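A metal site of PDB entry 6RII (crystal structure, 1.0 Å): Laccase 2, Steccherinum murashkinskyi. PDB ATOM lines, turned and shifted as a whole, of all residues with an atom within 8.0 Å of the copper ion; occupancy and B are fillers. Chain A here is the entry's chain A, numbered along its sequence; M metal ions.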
ATOM      1  N   CYS A 208       1.268   1.567 -29.442  1.00  0.00           N
ATOM      2  CA  CYS A 208       1.047   2.052 -28.073  1.00  0.00           C
ATOM      3  C   CYS A 208      -0.413   2.091 -27.695  1.00  0.00           C
ATOM      4  O   CYS A 208      -0.713   2.278 -26.507  1.00  0.00           O
ATOM      5  CB  CYS A 208       1.641   3.429 -27.848  1.00  0.00           C
ATOM      6  SG  CYS A 208       3.330   3.306 -27.179  1.00  0.00           S
ATOM      7  N   ASP A 209      -1.340   1.971 -28.643  1.00  0.00           N
ATOM      8  CA  ASP A 209      -2.764   2.154 -28.317  1.00  0.00           C
ATOM      9  C   ASP A 209      -3.687   1.518 -29.333  1.00  0.00           C
ATOM     10  O   ASP A 209      -4.311   0.509 -29.024  1.00  0.00           O
ATOM     11  CB  ASP A 209      -3.060   3.618 -28.032  1.00  0.00           C
ATOM     12  CG  ASP A 209      -4.502   3.953 -27.835  1.00  0.00           C
ATOM     13  OD1 ASP A 209      -5.372   3.146 -27.985  1.00  0.00           O
ATOM     14  OD2 ASP A 209      -4.759   5.184 -27.591  1.00  0.00           O
ATOM     15  N   PHE A 341      -6.598   3.827 -13.784  1.00  0.00           N
ATOM     16  CA  PHE A 341      -7.074   2.470 -13.815  1.00  0.00           C
ATOM     17  C   PHE A 341      -6.752   1.757 -12.526  1.00  0.00           C
ATOM     18  O   PHE A 341      -5.808   2.096 -11.812  1.00  0.00           O
ATOM     19  CB  PHE A 341      -6.417   1.728 -14.985  1.00  0.00           C
ATOM     20  CG  PHE A 341      -6.914   2.128 -16.315  1.00  0.00           C
ATOM     21  CD1 PHE A 341      -6.289   3.133 -17.023  1.00  0.00           C
ATOM     22  CD2 PHE A 341      -8.038   1.548 -16.871  1.00  0.00           C
ATOM     23  CE1 PHE A 341      -6.754   3.542 -18.264  1.00  0.00           C
ATOM     24  CE2 PHE A 341      -8.512   1.937 -18.104  1.00  0.00           C
ATOM     25  CZ  PHE A 341      -7.880   2.952 -18.804  1.00  0.00           C
ATOM     26  N   ALA A 392     -14.390  -1.335 -18.259  1.00  0.00           N
ATOM     27  CA  ALA A 392     -13.592  -0.143 -17.965  1.00  0.00           C
ATOM     28  C   ALA A 392     -13.427   0.722 -19.209  1.00  0.00           C
ATOM     29  O   ALA A 392     -13.163   0.165 -20.305  1.00  0.00           O
ATOM     30  CB  ALA A 392     -12.214  -0.536 -17.453  1.00  0.00           C
ATOM     31  N   ALA A 393     -13.537   2.035 -19.053  1.00  0.00           N
ATOM     32  CA  ALA A 393     -13.387   2.976 -20.168  1.00  0.00           C
ATOM     33  C   ALA A 393     -12.076   2.776 -20.900  1.00  0.00           C
ATOM     34  O   ALA A 393     -11.086   2.296 -20.362  1.00  0.00           O
ATOM     35  CB  ALA A 393     -13.475   4.391 -19.622  1.00  0.00           C
ATOM     36  N   GLY A 394     -12.104   3.214 -22.167  1.00  0.00           N
ATOM     37  CA  GLY A 394     -10.922   3.181 -22.995  1.00  0.00           C
ATOM     38  C   GLY A 394     -10.687   1.879 -23.732  1.00  0.00           C
ATOM     39  O   GLY A 394      -9.641   1.712 -24.346  1.00  0.00           O
ATOM     40  N   GLY A 395     -11.636   0.962 -23.673  1.00  0.00           N
ATOM     41  CA  GLY A 395     -11.478  -0.328 -24.313  1.00  0.00           C
ATOM     42  C   GLY A 395     -11.665  -0.264 -25.802  1.00  0.00           C
ATOM     43  O   GLY A 395     -12.025   0.772 -26.380  1.00  0.00           O
ATOM     44  N   PRO A 396     -11.470  -1.397 -26.500  1.00  0.00           N
ATOM     45  CA  PRO A 396     -11.177  -2.730 -25.914  1.00  0.00           C
ATOM     46  C   PRO A 396      -9.726  -2.833 -25.506  1.00  0.00           C
ATOM     47  O   PRO A 396      -8.784  -2.451 -26.215  1.00  0.00           O
ATOM     48  CB  PRO A 396     -11.479  -3.679 -27.061  1.00  0.00           C
ATOM     49  CG  PRO A 396     -11.293  -2.837 -28.303  1.00  0.00           C
ATOM     50  CD  PRO A 396     -11.699  -1.476 -27.949  1.00  0.00           C
ATOM     51  N   HIS A 397      -9.520  -3.357 -24.299  1.00  0.00           N
ATOM     52  CA  HIS A 397      -8.182  -3.430 -23.675  1.00  0.00           C
ATOM     53  C   HIS A 397      -7.475  -4.722 -24.036  1.00  0.00           C
ATOM     54  O   HIS A 397      -7.988  -5.796 -23.715  1.00  0.00           O
ATOM     55  CB  HIS A 397      -8.282  -3.322 -22.159  1.00  0.00           C
ATOM     56  CG  HIS A 397      -8.989  -2.074 -21.690  1.00  0.00           C
ATOM     57  ND1 HIS A 397      -8.341  -0.859 -21.670  1.00  0.00           N
ATOM     58  CD2 HIS A 397     -10.246  -1.909 -21.212  1.00  0.00           C
ATOM     59  CE1 HIS A 397      -9.216   0.024 -21.239  1.00  0.00           C
ATOM     60  NE2 HIS A 397     -10.357  -0.570 -20.933  1.00  0.00           N
ATOM     61  N   PRO A 398      -6.266  -4.662 -24.626  1.00  0.00           N
ATOM     62  CA  PRO A 398      -5.496  -5.864 -24.920  1.00  0.00           C
ATOM     63  C   PRO A 398      -4.595  -6.220 -23.738  1.00  0.00           C
ATOM     64  O   PRO A 398      -3.525  -5.646 -23.542  1.00  0.00           O
ATOM     65  CB  PRO A 398      -4.700  -5.454 -26.160  1.00  0.00           C
ATOM     66  CG  PRO A 398      -4.464  -3.966 -25.965  1.00  0.00           C
ATOM     67  CD  PRO A 398      -5.673  -3.463 -25.239  1.00  0.00           C
ATOM     68  N   PHE A 399      -5.018  -7.180 -22.938  1.00  0.00           N
ATOM     69  CA  PHE A 399      -4.255  -7.620 -21.790  1.00  0.00           C
ATOM     70  C   PHE A 399      -3.173  -8.586 -22.168  1.00  0.00           C
ATOM     71  O   PHE A 399      -3.349  -9.507 -22.968  1.00  0.00           O
ATOM     72  CB  PHE A 399      -5.170  -8.206 -20.693  1.00  0.00           C
ATOM     73  CG  PHE A 399      -5.602  -7.188 -19.702  1.00  0.00           C
ATOM     74  CD1 PHE A 399      -6.487  -6.163 -20.029  1.00  0.00           C
ATOM     75  CD2 PHE A 399      -5.018  -7.152 -18.412  1.00  0.00           C
ATOM     76  CE1 PHE A 399      -6.796  -5.158 -19.117  1.00  0.00           C
ATOM     77  CE2 PHE A 399      -5.338  -6.142 -17.526  1.00  0.00           C
ATOM     78  CZ  PHE A 399      -6.207  -5.156 -17.865  1.00  0.00           C
ATOM     79  N   ILE A 430      -9.880  -7.979 -24.267  1.00  0.00           N
ATOM     80  CA  ILE A 430     -10.932  -8.385 -23.305  1.00  0.00           C
ATOM     81  C   ILE A 430     -12.312  -7.938 -23.754  1.00  0.00           C
ATOM     82  O   ILE A 430     -13.311  -8.237 -23.092  1.00  0.00           O
ATOM     83  CB  ILE A 430     -10.599  -7.979 -21.875  1.00  0.00           C
ATOM     84  CG1 ILE A 430     -10.701  -6.465 -21.656  1.00  0.00           C
ATOM     85  CG2 ILE A 430      -9.244  -8.535 -21.467  1.00  0.00           C
ATOM     86  CD1 ILE A 430     -10.613  -6.061 -20.200  1.00  0.00           C
ATOM     87  N   HIS A 452      -0.838  -6.740 -17.630  1.00  0.00           N
ATOM     88  CA  HIS A 452      -1.304  -5.372 -17.811  1.00  0.00           C
ATOM     89  C   HIS A 452      -1.960  -5.192 -19.134  1.00  0.00           C
ATOM     90  O   HIS A 452      -1.751  -5.938 -20.091  1.00  0.00           O
ATOM     91  CB  HIS A 452      -0.124  -4.376 -17.666  1.00  0.00           C
ATOM     92  CG  HIS A 452       0.964  -4.544 -18.664  1.00  0.00           C
ATOM     93  ND1 HIS A 452       0.948  -3.936 -19.899  1.00  0.00           N
ATOM     94  CD2 HIS A 452       2.134  -5.231 -18.596  1.00  0.00           C
ATOM     95  CE1 HIS A 452       2.075  -4.281 -20.531  1.00  0.00           C
ATOM     96  NE2 HIS A 452       2.834  -5.080 -19.770  1.00  0.00           N
ATOM     97  N   CYS A 453      -2.752  -4.107 -19.232  1.00  0.00           N
ATOM     98  CA  CYS A 453      -3.217  -3.658 -20.537  1.00  0.00           C
ATOM     99  C   CYS A 453      -2.015  -3.147 -21.318  1.00  0.00           C
ATOM    100  O   CYS A 453      -1.193  -2.413 -20.794  1.00  0.00           O
ATOM    101  CB  CYS A 453      -4.223  -2.528 -20.349  1.00  0.00           C
ATOM    102  SG  CYS A 453      -4.836  -2.001 -21.997  1.00  0.00           S
ATOM    103  N   HIS A 454      -1.926  -3.527 -22.596  1.00  0.00           N
ATOM    104  CA  HIS A 454      -0.809  -3.129 -23.446  1.00  0.00           C
ATOM    105  C   HIS A 454      -1.073  -1.840 -24.209  1.00  0.00           C
ATOM    106  O   HIS A 454      -0.233  -1.432 -25.010  1.00  0.00           O
ATOM    107  CB  HIS A 454      -0.378  -4.269 -24.379  1.00  0.00           C
ATOM    108  CG  HIS A 454       1.105  -4.317 -24.606  1.00  0.00           C
ATOM    109  ND1 HIS A 454       1.804  -3.304 -25.219  1.00  0.00           N
ATOM    110  CD2 HIS A 454       2.020  -5.271 -24.343  1.00  0.00           C
ATOM    111  CE1 HIS A 454       3.090  -3.659 -25.260  1.00  0.00           C
ATOM    112  NE2 HIS A 454       3.266  -4.849 -24.754  1.00  0.00           N
ATOM    113  N   ILE A 455      -2.173  -1.152 -23.925  1.00  0.00           N
ATOM    114  CA  ILE A 455      -2.283   0.262 -24.328  1.00  0.00           C
ATOM    115  C   ILE A 455      -1.391   1.003 -23.342  1.00  0.00           C
ATOM    116  O   ILE A 455      -1.659   1.051 -22.130  1.00  0.00           O
ATOM    117  CB  ILE A 455      -3.743   0.735 -24.309  1.00  0.00           C
ATOM    118  CG1 ILE A 455      -4.538   0.011 -25.379  1.00  0.00           C
ATOM    119  CG2 ILE A 455      -3.787   2.256 -24.487  1.00  0.00           C
ATOM    120  CD1 ILE A 455      -6.039   0.164 -25.282  1.00  0.00           C
ATOM    121  N   ASP A 456      -0.282   1.538 -23.846  1.00  0.00           N
ATOM    122  CA  ASP A 456       0.782   1.990 -22.937  1.00  0.00           C
ATOM    123  C   ASP A 456       0.316   3.148 -22.072  1.00  0.00           C
ATOM    124  O   ASP A 456       0.756   3.290 -20.928  1.00  0.00           O
ATOM    125  CB  ASP A 456       2.036   2.319 -23.749  1.00  0.00           C
ATOM    126  CG  ASP A 456       3.343   2.054 -23.005  1.00  0.00           C
ATOM    127  OD1 ASP A 456       3.383   1.070 -22.258  1.00  0.00           O
ATOM    128  OD2 ASP A 456       4.290   2.807 -23.231  1.00  0.00           O
ATOM    129  N   TRP A 457      -0.596   3.971 -22.585  1.00  0.00           N
ATOM    130  CA  TRP A 457      -1.141   5.063 -21.822  1.00  0.00           C
ATOM    131  C   TRP A 457      -1.936   4.534 -20.602  1.00  0.00           C
ATOM    132  O   TRP A 457      -2.026   5.211 -19.576  1.00  0.00           O
ATOM    133  CB  TRP A 457      -2.033   5.943 -22.714  1.00  0.00           C
ATOM    134  CG  TRP A 457      -1.392   6.306 -24.030  1.00  0.00           C
ATOM    135  CD1 TRP A 457      -1.793   5.899 -25.267  1.00  0.00           C
ATOM    136  CD2 TRP A 457      -0.242   7.115 -24.224  1.00  0.00           C
ATOM    137  NE1 TRP A 457      -0.955   6.370 -26.220  1.00  0.00           N
ATOM    138  CE2 TRP A 457       0.017   7.125 -25.632  1.00  0.00           C
ATOM    139  CE3 TRP A 457       0.590   7.846 -23.386  1.00  0.00           C
ATOM    140  CZ2 TRP A 457       1.068   7.825 -26.176  1.00  0.00           C
ATOM    141  CZ3 TRP A 457       1.629   8.525 -23.944  1.00  0.00           C
ATOM    142  CH2 TRP A 457       1.861   8.516 -25.313  1.00  0.00           C
ATOM    143  N   HIS A 458      -2.544   3.368 -20.762  1.00  0.00           N
ATOM    144  CA  HIS A 458      -3.329   2.768 -19.676  1.00  0.00           C
ATOM    145  C   HIS A 458      -2.433   2.104 -18.639  1.00  0.00           C
ATOM    146  O   HIS A 458      -2.692   2.201 -17.438  1.00  0.00           O
ATOM    147  CB  HIS A 458      -4.332   1.754 -20.257  1.00  0.00           C
ATOM    148  CG  HIS A 458      -5.336   2.348 -21.174  1.00  0.00           C
ATOM    149  ND1 HIS A 458      -6.258   1.534 -21.817  1.00  0.00           N
ATOM    150  CD2 HIS A 458      -5.560   3.628 -21.527  1.00  0.00           C
ATOM    151  CE1 HIS A 458      -7.000   2.369 -22.548  1.00  0.00           C
ATOM    152  NE2 HIS A 458      -6.604   3.626 -22.390  1.00  0.00           N
ATOM    153  N   LEU A 459      -1.361   1.426 -19.088  1.00  0.00           N
ATOM    154  CA  LEU A 459      -0.356   0.925 -18.170  1.00  0.00           C
ATOM    155  C   LEU A 459       0.171   2.066 -17.319  1.00  0.00           C
ATOM    156  O   LEU A 459       0.282   1.949 -16.071  1.00  0.00           O
ATOM    157  CB  LEU A 459       0.752   0.238 -18.955  1.00  0.00           C
ATOM    158  CG  LEU A 459       1.979  -0.134 -18.148  1.00  0.00           C
ATOM    159  CD1 LEU A 459       1.680  -1.040 -16.979  1.00  0.00           C
ATOM    160  CD2 LEU A 459       3.037  -0.750 -19.039  1.00  0.00           C
ATOM    161  N   PHE A 463      -2.987   0.408 -15.015  1.00  0.00           N
ATOM    162  CA  PHE A 463      -3.808  -0.805 -15.358  1.00  0.00           C
ATOM    163  C   PHE A 463      -2.930  -2.060 -15.380  1.00  0.00           C
ATOM    164  O   PHE A 463      -2.670  -2.634 -16.446  1.00  0.00           O
ATOM    165  CB  PHE A 463      -4.538  -0.578 -16.657  1.00  0.00           C
ATOM    166  CG  PHE A 463      -5.893  -1.241 -16.802  1.00  0.00           C
ATOM    167  CD1 PHE A 463      -6.597  -1.784 -15.732  1.00  0.00           C
ATOM    168  CD2 PHE A 463      -6.525  -1.222 -18.047  1.00  0.00           C
ATOM    169  CE1 PHE A 463      -7.878  -2.256 -15.891  1.00  0.00           C
ATOM    170  CE2 PHE A 463      -7.804  -1.703 -18.224  1.00  0.00           C
ATOM    171  CZ  PHE A 463      -8.489  -2.214 -17.133  1.00  0.00           C
HETATM  172 CU    CU M   1      -6.356  -0.450 -21.783  1.00  0.00          CU
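The backbone NH (N) of Phe 463 lies within hydrogen-bond range of the backbone carbonyl oxygen (O) of His 458, at 3.0 Å.
NE2 of His 397 is in hydrogen-bond range of O of Ala 393, at 3.0 Å.
The backbone NH (N) of Gly 395 lies within hydrogen-bond range of a ring nitrogen (NE2) of His 397 (3.4 Å).
NE2 of His 397 lies within hydrogen-bond range of O of Ala 392, at 3.0 Å.
N of Ile 430 lies within hydrogen-bond range of O of His 397 (2.9 Å).
SG of Cys 453 lies close to N of Ile 455 (3.4 Å).
O of Phe 463 is in hydrogen-bond range of N of Cys 453.
Ile 455 touches the copper ion (CD1 to CU, 3.6 Å).
Phe 463 touches the copper ion.
Five residues have an atom within 4 Å of the copper ion: His 397, Cys 453, Ile 455, His 458 and Phe 463.
Along chain A the residues within 4 Å of the copper ion span positions 397 to 463.
The nearest printed residue that does not touch the copper ion is Pro 398 (4.6 Å).
The copper ion is bound by a ring nitrogen (ND1) of His 458, at 2.0 Å.
ND1 of His 397 binds the copper ion, at 2.0 Å.
The copper ion is bound by the side-chain sulfur (SG) of Cys 453.
The copper ion has three donor atoms within binding distance.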
